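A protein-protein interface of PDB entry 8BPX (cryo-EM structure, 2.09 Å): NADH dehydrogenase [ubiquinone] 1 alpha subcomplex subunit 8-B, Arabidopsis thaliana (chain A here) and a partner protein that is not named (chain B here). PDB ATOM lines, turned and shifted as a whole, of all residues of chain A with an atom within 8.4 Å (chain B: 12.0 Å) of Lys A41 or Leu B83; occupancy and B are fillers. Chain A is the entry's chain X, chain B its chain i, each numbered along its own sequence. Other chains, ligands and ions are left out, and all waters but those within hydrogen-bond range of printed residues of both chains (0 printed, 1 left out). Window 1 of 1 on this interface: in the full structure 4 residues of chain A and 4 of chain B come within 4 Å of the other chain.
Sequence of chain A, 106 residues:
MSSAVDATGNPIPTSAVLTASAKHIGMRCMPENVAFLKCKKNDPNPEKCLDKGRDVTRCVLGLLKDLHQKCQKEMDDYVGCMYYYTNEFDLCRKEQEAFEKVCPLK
The side-chain carboxylate (OD1) of Asp B80 lies within salt-bridge range of the side-chain amino group (NZ) of Lys A41 (3.0 Å).
The side-chain carboxylate (OD2) of Asp B80 sits at hydrogen-bond distance from the backbone NH (N) of Asp B77.
Among the printed residues, pairs that only touch across the chains: Lys A40 with Tyr B79 (3.4 Å), Lys A41 with Leu B83 (3.5 Å), Leu A37 with Leu B83 (3.6 Å), Lys A38 with Leu B83 (3.7 Å) and Leu A37 with Leu B82 (3.7 Å).
Of chain B, only Asp B80 (3.0 Å) and Leu B83 (3.5 Å) come within 4 Å of Lys A41. Of chain A, only Leu A37 (3.6 Å), Lys A38 (3.7 Å) and Lys A41 (3.5 Å) come within 4 Å of Leu B83. No residue of chain B comes within 4 Å of Val A34. Printed residues of chain B within 4 Å of Leu A37: Leu B82 and Leu B83. Of chain B, only Leu B83 comes within 4 Å of Lys A38. No residue of chain B comes within 4 Å of Cys A39. Lys A40 touches just one residue of chain B: Tyr B79. Printed residues of chain A within 4 Å of Leu B82: Leu A37 (3.7 Å). Of the printed residues of chain A, Tyr B79 touches Lys A40. Printed residues of chain A within 4 Å of Asp B80: Lys A41 (3.0 Å). Pro A44 touches none of the printed residues of chain B. Phe A36 touches none of the printed residues of chain B. The nearest residue of chain A that does not touch Leu B83 is Val A34 (4.1 Å). The nearest printed residue of chain A that does not touch Tyr B79 is Lys A41 (4.3 Å).
Printed residues of chain A that touch a printed residue of chain B: Leu A37, Lys A38, Lys A40 and Lys A41. Hydrophobic or aromatic side chains of chain A within 4 Å of the printed part of chain B: Leu A37. Along chain A the printed residues that touch a printed residue of chain B span positions 37 to 41.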
ATOM      1  N   MET A  30       5.303  14.617  11.948  1.00  0.00           N
ATOM      2  CA  MET A  30       3.975  14.252  12.438  1.00  0.00           C
ATOM      3  C   MET A  30       2.920  15.325  12.188  1.00  0.00           C
ATOM      4  O   MET A  30       1.836  14.981  11.686  1.00  0.00           O
ATOM      5  CB  MET A  30       4.059  13.889  13.925  1.00  0.00           C
ATOM      6  CG  MET A  30       2.816  13.220  14.472  1.00  0.00           C
ATOM      7  SD  MET A  30       2.482  11.640  13.672  1.00  0.00           S
ATOM      8  CE  MET A  30       1.005  11.122  14.543  1.00  0.00           C
ATOM      9  N   PRO A  31       3.138  16.609  12.515  1.00  0.00           N
ATOM     10  CA  PRO A  31       2.071  17.599  12.270  1.00  0.00           C
ATOM     11  C   PRO A  31       1.678  17.723  10.809  1.00  0.00           C
ATOM     12  O   PRO A  31       0.481  17.761  10.497  1.00  0.00           O
ATOM     13  CB  PRO A  31       2.678  18.904  12.810  1.00  0.00           C
ATOM     14  CG  PRO A  31       3.698  18.471  13.787  1.00  0.00           C
ATOM     15  CD  PRO A  31       4.284  17.217  13.217  1.00  0.00           C
ATOM     16  N   ASN A  33       2.000  15.442   8.473  1.00  0.00           N
ATOM     17  CA  ASN A  33       1.314  14.204   8.115  1.00  0.00           C
ATOM     18  C   ASN A  33      -0.141  14.237   8.566  1.00  0.00           C
ATOM     19  O   ASN A  33      -1.054  13.937   7.788  1.00  0.00           O
ATOM     20  CB  ASN A  33       2.038  13.007   8.740  1.00  0.00           C
ATOM     21  CG  ASN A  33       3.240  12.551   7.929  1.00  0.00           C
ATOM     22  OD1 ASN A  33       3.490  13.041   6.830  1.00  0.00           O
ATOM     23  ND2 ASN A  33       3.994  11.608   8.478  1.00  0.00           N
ATOM     24  N   VAL A  34      -0.372  14.608   9.828  1.00  0.00           N
ATOM     25  CA  VAL A  34      -1.731  14.628  10.362  1.00  0.00           C
ATOM     26  C   VAL A  34      -2.584  15.649   9.621  1.00  0.00           C
ATOM     27  O   VAL A  34      -3.751  15.389   9.310  1.00  0.00           O
ATOM     28  CB  VAL A  34      -1.707  14.894  11.878  1.00  0.00           C
ATOM     29  CG1 VAL A  34      -3.121  15.032  12.416  1.00  0.00           C
ATOM     30  CG2 VAL A  34      -0.975  13.780  12.593  1.00  0.00           C
ATOM     31  N   ALA A  35      -2.022  16.823   9.323  1.00  0.00           N
ATOM     32  CA  ALA A  35      -2.776  17.844   8.601  1.00  0.00           C
ATOM     33  C   ALA A  35      -3.167  17.362   7.208  1.00  0.00           C
ATOM     34  O   ALA A  35      -4.314  17.536   6.771  1.00  0.00           O
ATOM     35  CB  ALA A  35      -1.955  19.130   8.512  1.00  0.00           C
ATOM     36  N   PHE A  36      -2.217  16.747   6.499  1.00  0.00           N
ATOM     37  CA  PHE A  36      -2.503  16.194   5.182  1.00  0.00           C
ATOM     38  C   PHE A  36      -3.609  15.150   5.259  1.00  0.00           C
ATOM     39  O   PHE A  36      -4.519  15.128   4.422  1.00  0.00           O
ATOM     40  CB  PHE A  36      -1.231  15.586   4.590  1.00  0.00           C
ATOM     41  CG  PHE A  36      -1.421  14.974   3.233  1.00  0.00           C
ATOM     42  CD1 PHE A  36      -1.429  15.761   2.095  1.00  0.00           C
ATOM     43  CD2 PHE A  36      -1.595  13.604   3.097  1.00  0.00           C
ATOM     44  CE1 PHE A  36      -1.599  15.193   0.847  1.00  0.00           C
ATOM     45  CE2 PHE A  36      -1.771  13.035   1.851  1.00  0.00           C
ATOM     46  CZ  PHE A  36      -1.773  13.832   0.725  1.00  0.00           C
ATOM     47  N   LEU A  37      -3.538  14.267   6.257  1.00  0.00           N
ATOM     48  CA  LEU A  37      -4.540  13.212   6.370  1.00  0.00           C
ATOM     49  C   LEU A  37      -5.916  13.776   6.706  1.00  0.00           C
ATOM     50  O   LEU A  37      -6.925  13.296   6.184  1.00  0.00           O
ATOM     51  CB  LEU A  37      -4.105  12.176   7.403  1.00  0.00           C
ATOM     52  CG  LEU A  37      -2.829  11.425   7.023  1.00  0.00           C
ATOM     53  CD1 LEU A  37      -2.410  10.467   8.120  1.00  0.00           C
ATOM     54  CD2 LEU A  37      -3.032  10.697   5.705  1.00  0.00           C
ATOM     55  N   LYS A  38      -5.982  14.793   7.568  1.00  0.00           N
ATOM     56  CA  LYS A  38      -7.264  15.443   7.831  1.00  0.00           C
ATOM     57  C   LYS A  38      -7.847  16.029   6.553  1.00  0.00           C
ATOM     58  O   LYS A  38      -9.032  15.830   6.246  1.00  0.00           O
ATOM     59  CB  LYS A  38      -7.111  16.536   8.893  1.00  0.00           C
ATOM     60  CG  LYS A  38      -6.563  16.072  10.222  1.00  0.00           C
ATOM     61  CD  LYS A  38      -7.177  16.850  11.374  1.00  0.00           C
ATOM     62  CE  LYS A  38      -6.155  17.114  12.465  1.00  0.00           C
ATOM     63  NZ  LYS A  38      -6.395  16.273  13.668  1.00  0.00           N
ATOM     64  N   CYS A  39      -7.024  16.741   5.778  1.00  0.00           N
ATOM     65  CA  CYS A  39      -7.550  17.373   4.572  1.00  0.00           C
ATOM     66  C   CYS A  39      -7.998  16.326   3.557  1.00  0.00           C
ATOM     67  O   CYS A  39      -9.025  16.499   2.892  1.00  0.00           O
ATOM     68  CB  CYS A  39      -6.512  18.316   3.966  1.00  0.00           C
ATOM     69  SG  CYS A  39      -6.820  18.723   2.243  1.00  0.00           S
ATOM     70  N   LYS A  40      -7.247  15.226   3.437  1.00  0.00           N
ATOM     71  CA  LYS A  40      -7.665  14.126   2.571  1.00  0.00           C
ATOM     72  C   LYS A  40      -8.973  13.512   3.052  1.00  0.00           C
ATOM     73  O   LYS A  40      -9.830  13.147   2.239  1.00  0.00           O
ATOM     74  CB  LYS A  40      -6.566  13.061   2.502  1.00  0.00           C
ATOM     75  CG  LYS A  40      -5.395  13.417   1.600  1.00  0.00           C
ATOM     76  CD  LYS A  40      -5.872  13.910   0.243  1.00  0.00           C
ATOM     77  CE  LYS A  40      -6.323  12.764  -0.643  1.00  0.00           C
ATOM     78  NZ  LYS A  40      -5.887  12.951  -2.053  1.00  0.00           N
ATOM     79  N   LYS A  41      -9.140  13.383   4.371  1.00  0.00           N
ATOM     80  CA  LYS A  41     -10.397  12.891   4.924  1.00  0.00           C
ATOM     81  C   LYS A  41     -11.564  13.778   4.522  1.00  0.00           C
ATOM     82  O   LYS A  41     -12.635  13.279   4.157  1.00  0.00           O
ATOM     83  CB  LYS A  41     -10.305  12.806   6.448  1.00  0.00           C
ATOM     84  CG  LYS A  41     -11.266  11.820   7.073  1.00  0.00           C
ATOM     85  CD  LYS A  41     -10.804  11.388   8.448  1.00  0.00           C
ATOM     86  CE  LYS A  41     -11.976  10.951   9.312  1.00  0.00           C
ATOM     87  NZ  LYS A  41     -13.051  10.314   8.509  1.00  0.00           N
ATOM     88  N   ASN A  42     -11.385  15.098   4.591  1.00  0.00           N
ATOM     89  CA  ASN A  42     -12.478  15.994   4.223  1.00  0.00           C
ATOM     90  C   ASN A  42     -12.707  15.999   2.715  1.00  0.00           C
ATOM     91  O   ASN A  42     -13.855  16.034   2.256  1.00  0.00           O
ATOM     92  CB  ASN A  42     -12.201  17.404   4.755  1.00  0.00           C
ATOM     93  CG  ASN A  42     -13.360  18.366   4.541  1.00  0.00           C
ATOM     94  OD1 ASN A  42     -14.231  18.148   3.699  1.00  0.00           O
ATOM     95  ND2 ASN A  42     -13.370  19.447   5.312  1.00  0.00           N
ATOM     96  N   ASP A  43     -11.636  15.962   1.929  1.00  0.00           N
ATOM     97  CA  ASP A  43     -11.785  16.071   0.484  1.00  0.00           C
ATOM     98  C   ASP A  43     -10.808  15.163  -0.253  1.00  0.00           C
ATOM     99  O   ASP A  43      -9.591  15.378  -0.196  1.00  0.00           O
ATOM    100  CB  ASP A  43     -11.589  17.520   0.040  1.00  0.00           C
ATOM    101  CG  ASP A  43     -12.625  17.964  -0.969  1.00  0.00           C
ATOM    102  OD1 ASP A  43     -13.047  17.125  -1.787  1.00  0.00           O
ATOM    103  OD2 ASP A  43     -13.013  19.149  -0.942  1.00  0.00           O
ATOM    104  N   PRO A  44     -11.301  14.142  -0.959  1.00  0.00           N
ATOM    105  CA  PRO A  44     -10.406  13.271  -1.733  1.00  0.00           C
ATOM    106  C   PRO A  44      -9.916  13.877  -3.038  1.00  0.00           C
ATOM    107  O   PRO A  44      -9.051  13.273  -3.686  1.00  0.00           O
ATOM    108  CB  PRO A  44     -11.276  12.038  -2.000  1.00  0.00           C
ATOM    109  CG  PRO A  44     -12.660  12.589  -2.039  1.00  0.00           C
ATOM    110  CD  PRO A  44     -12.696  13.673  -0.999  1.00  0.00           C
ATOM    111  N   ASN A  45     -10.437  15.026  -3.450  1.00  0.00           N
ATOM    112  CA  ASN A  45     -10.003  15.639  -4.697  1.00  0.00           C
ATOM    113  C   ASN A  45      -8.538  16.044  -4.578  1.00  0.00           C
ATOM    114  O   ASN A  45      -8.193  16.846  -3.697  1.00  0.00           O
ATOM    115  CB  ASN A  45     -10.875  16.851  -5.024  1.00  0.00           C
ATOM    116  CG  ASN A  45     -10.612  17.413  -6.413  1.00  0.00           C
ATOM    117  OD1 ASN A  45      -9.824  16.868  -7.184  1.00  0.00           O
ATOM    118  ND2 ASN A  45     -11.287  18.502  -6.743  1.00  0.00           N
ATOM    119  N   CYS A  49      -5.773  19.670  -2.217  1.00  0.00           N
ATOM    120  CA  CYS A  49      -4.909  19.240  -1.123  1.00  0.00           C
ATOM    121  C   CYS A  49      -3.432  19.477  -1.425  1.00  0.00           C
ATOM    122  O   CYS A  49      -2.577  19.051  -0.638  1.00  0.00           O
ATOM    123  CB  CYS A  49      -5.167  17.756  -0.817  1.00  0.00           C
ATOM    124  SG  CYS A  49      -4.388  17.080   0.666  1.00  0.00           S
ATOM    125  N   SER B  70     -20.701   1.702  11.659  1.00  0.00           N
ATOM    126  CA  SER B  70     -19.893   2.494  10.740  1.00  0.00           C
ATOM    127  C   SER B  70     -18.402   2.423  11.048  1.00  0.00           C
ATOM    128  O   SER B  70     -17.590   2.761  10.182  1.00  0.00           O
ATOM    129  CB  SER B  70     -20.365   3.952  10.755  1.00  0.00           C
ATOM    130  OG  SER B  70     -20.056   4.573  11.987  1.00  0.00           O
ATOM    131  N   GLN B  71     -18.024   1.995  12.249  1.00  0.00           N
ATOM    132  CA  GLN B  71     -16.626   1.867  12.635  1.00  0.00           C
ATOM    133  C   GLN B  71     -16.131   0.426  12.568  1.00  0.00           C
ATOM    134  O   GLN B  71     -15.043   0.132  13.068  1.00  0.00           O
ATOM    135  CB  GLN B  71     -16.418   2.428  14.044  1.00  0.00           C
ATOM    136  CG  GLN B  71     -16.092   3.913  14.091  1.00  0.00           C
ATOM    137  CD  GLN B  71     -16.703   4.686  12.939  1.00  0.00           C
ATOM    138  OE1 GLN B  71     -17.915   4.884  12.881  1.00  0.00           O
ATOM    139  NE2 GLN B  71     -15.863   5.118  12.010  1.00  0.00           N
ATOM    140  N   VAL B  72     -16.904  -0.471  11.966  1.00  0.00           N
ATOM    141  CA  VAL B  72     -16.563  -1.889  11.938  1.00  0.00           C
ATOM    142  C   VAL B  72     -15.583  -2.152  10.804  1.00  0.00           C
ATOM    143  O   VAL B  72     -15.782  -1.692   9.673  1.00  0.00           O
ATOM    144  CB  VAL B  72     -17.832  -2.744  11.793  1.00  0.00           C
ATOM    145  CG1 VAL B  72     -17.476  -4.179  11.438  1.00  0.00           C
ATOM    146  CG2 VAL B  72     -18.659  -2.685  13.068  1.00  0.00           C
ATOM    147  N   ARG B  75     -15.885  -2.026   6.499  1.00  0.00           N
ATOM    148  CA  ARG B  75     -16.727  -1.024   5.855  1.00  0.00           C
ATOM    149  C   ARG B  75     -16.305   0.402   6.202  1.00  0.00           C
ATOM    150  O   ARG B  75     -17.086   1.336   5.991  1.00  0.00           O
ATOM    151  CB  ARG B  75     -18.203  -1.239   6.220  1.00  0.00           C
ATOM    152  CG  ARG B  75     -18.513  -1.112   7.700  1.00  0.00           C
ATOM    153  CD  ARG B  75     -19.894  -1.655   8.024  1.00  0.00           C
ATOM    154  NE  ARG B  75     -20.961  -0.805   7.513  1.00  0.00           N
ATOM    155  CZ  ARG B  75     -21.732  -1.108   6.478  1.00  0.00           C
ATOM    156  NH1 ARG B  75     -21.577  -2.241   5.810  1.00  0.00           N
ATOM    157  NH2 ARG B  75     -22.679  -0.256   6.103  1.00  0.00           N
ATOM    158  N   ARG B  76     -15.096   0.594   6.711  1.00  0.00           N
ATOM    159  CA  ARG B  76     -14.608   1.914   7.079  1.00  0.00           C
ATOM    160  C   ARG B  76     -13.962   2.615   5.890  1.00  0.00           C
ATOM    161  O   ARG B  76     -13.398   1.976   4.998  1.00  0.00           O
ATOM    162  CB  ARG B  76     -13.599   1.809   8.220  1.00  0.00           C
ATOM    163  CG  ARG B  76     -14.077   0.950   9.364  1.00  0.00           C
ATOM    164  CD  ARG B  76     -13.188   1.092  10.568  1.00  0.00           C
ATOM    165  NE  ARG B  76     -13.267   2.427  11.144  1.00  0.00           N
ATOM    166  CZ  ARG B  76     -12.372   2.928  11.984  1.00  0.00           C
ATOM    167  NH1 ARG B  76     -11.325   2.224  12.375  1.00  0.00           N
ATOM    168  NH2 ARG B  76     -12.534   4.166  12.438  1.00  0.00           N
ATOM    169  N   ASP B  77     -14.061   3.939   5.886  1.00  0.00           N
ATOM    170  CA  ASP B  77     -13.258   4.739   4.975  1.00  0.00           C
ATOM    171  C   ASP B  77     -11.785   4.490   5.288  1.00  0.00           C
ATOM    172  O   ASP B  77     -11.402   4.489   6.464  1.00  0.00           O
ATOM    173  CB  ASP B  77     -13.606   6.224   5.123  1.00  0.00           C
ATOM    174  CG  ASP B  77     -12.871   7.122   4.126  1.00  0.00           C
ATOM    175  OD1 ASP B  77     -12.094   6.618   3.291  1.00  0.00           O
ATOM    176  OD2 ASP B  77     -13.082   8.348   4.164  1.00  0.00           O
ATOM    177  N   PRO B  78     -10.938   4.259   4.280  1.00  0.00           N
ATOM    178  CA  PRO B  78      -9.528   3.947   4.569  1.00  0.00           C
ATOM    179  C   PRO B  78      -8.806   5.020   5.365  1.00  0.00           C
ATOM    180  O   PRO B  78      -7.870   4.696   6.105  1.00  0.00           O
ATOM    181  CB  PRO B  78      -8.914   3.765   3.171  1.00  0.00           C
ATOM    182  CG  PRO B  78      -9.923   4.309   2.208  1.00  0.00           C
ATOM    183  CD  PRO B  78     -11.251   4.103   2.852  1.00  0.00           C
ATOM    184  N   TYR B  79      -9.217   6.285   5.257  1.00  0.00           N
ATOM    185  CA  TYR B  79      -8.536   7.345   5.990  1.00  0.00           C
ATOM    186  C   TYR B  79      -8.854   7.341   7.484  1.00  0.00           C
ATOM    187  O   TYR B  79      -8.127   7.973   8.254  1.00  0.00           O
ATOM    188  CB  TYR B  79      -8.877   8.702   5.377  1.00  0.00           C
ATOM    189  CG  TYR B  79      -8.152   8.944   4.077  1.00  0.00           C
ATOM    190  CD1 TYR B  79      -6.770   9.072   4.051  1.00  0.00           C
ATOM    191  CD2 TYR B  79      -8.842   9.017   2.874  1.00  0.00           C
ATOM    192  CE1 TYR B  79      -6.096   9.281   2.868  1.00  0.00           C
ATOM    193  CE2 TYR B  79      -8.174   9.225   1.686  1.00  0.00           C
ATOM    194  CZ  TYR B  79      -6.802   9.357   1.689  1.00  0.00           C
ATOM    195  OH  TYR B  79      -6.129   9.566   0.512  1.00  0.00           O
ATOM    196  N   ASP B  80      -9.917   6.650   7.909  1.00  0.00           N
ATOM    197  CA  ASP B  80     -10.232   6.579   9.334  1.00  0.00           C
ATOM    198  C   ASP B  80      -9.143   5.865  10.123  1.00  0.00           C
ATOM    199  O   ASP B  80      -8.878   6.220  11.277  1.00  0.00           O
ATOM    200  CB  ASP B  80     -11.573   5.879   9.547  1.00  0.00           C
ATOM    201  CG  ASP B  80     -12.627   6.339   8.572  1.00  0.00           C
ATOM    202  OD1 ASP B  80     -12.448   7.424   7.989  1.00  0.00           O
ATOM    203  OD2 ASP B  80     -13.625   5.616   8.378  1.00  0.00           O
ATOM    204  N   ASP B  81      -8.507   4.855   9.529  1.00  0.00           N
ATOM    205  CA  ASP B  81      -7.444   4.145  10.228  1.00  0.00           C
ATOM    206  C   ASP B  81      -6.196   5.012  10.361  1.00  0.00           C
ATOM    207  O   ASP B  81      -5.492   4.941  11.375  1.00  0.00           O
ATOM    208  CB  ASP B  81      -7.126   2.839   9.506  1.00  0.00           C
ATOM    209  CG  ASP B  81      -7.024   1.661  10.453  1.00  0.00           C
ATOM    210  OD1 ASP B  81      -6.942   1.889  11.679  1.00  0.00           O
ATOM    211  OD2 ASP B  81      -7.026   0.508   9.974  1.00  0.00           O
ATOM    212  N   LEU B  82      -5.904   5.834   9.350  1.00  0.00           N
ATOM    213  CA  LEU B  82      -4.728   6.697   9.401  1.00  0.00           C
ATOM    214  C   LEU B  82      -4.833   7.764  10.482  1.00  0.00           C
ATOM    215  O   LEU B  82      -3.806   8.186  11.019  1.00  0.00           O
ATOM    216  CB  LEU B  82      -4.499   7.378   8.050  1.00  0.00           C
ATOM    217  CG  LEU B  82      -3.862   6.571   6.917  1.00  0.00           C
ATOM    218  CD1 LEU B  82      -2.724   5.729   7.450  1.00  0.00           C
ATOM    219  CD2 LEU B  82      -4.873   5.707   6.201  1.00  0.00           C
ATOM    220  N   LEU B  83      -6.043   8.212  10.805  1.00  0.00           N
ATOM    221  CA  LEU B  83      -6.229   9.280  11.776  1.00  0.00           C
ATOM    222  C   LEU B  83      -6.655   8.781  13.147  1.00  0.00           C
ATOM    223  O   LEU B  83      -6.679   9.574  14.093  1.00  0.00           O
ATOM    224  CB  LEU B  83      -7.256  10.287  11.251  1.00  0.00           C
ATOM    225  CG  LEU B  83      -6.662  11.247  10.220  1.00  0.00           C
ATOM    226  CD1 LEU B  83      -7.666  12.305   9.802  1.00  0.00           C
ATOM    227  CD2 LEU B  83      -5.406  11.890  10.774  1.00  0.00           C
ATOM    228  N   GLU B  84      -6.976   7.498  13.284  1.00  0.00           N
ATOM    229  CA  GLU B  84      -7.365   6.946  14.576  1.00  0.00           C
ATOM    230  C   GLU B  84      -6.308   5.976  15.094  1.00  0.00           C
ATOM    231  O   GLU B  84      -6.114   5.843  16.303  1.00  0.00           O
ATOM    232  CB  GLU B  84      -8.720   6.243  14.475  1.00  0.00           C
ATOM    233  CG  GLU B  84      -9.917   7.165  14.654  1.00  0.00           C
ATOM    234  CD  GLU B  84     -10.127   7.578  16.097  1.00  0.00           C
ATOM    235  OE1 GLU B  84      -9.854   6.756  16.999  1.00  0.00           O
ATOM    236  OE2 GLU B  84     -10.567   8.724  16.330  1.00  0.00           O
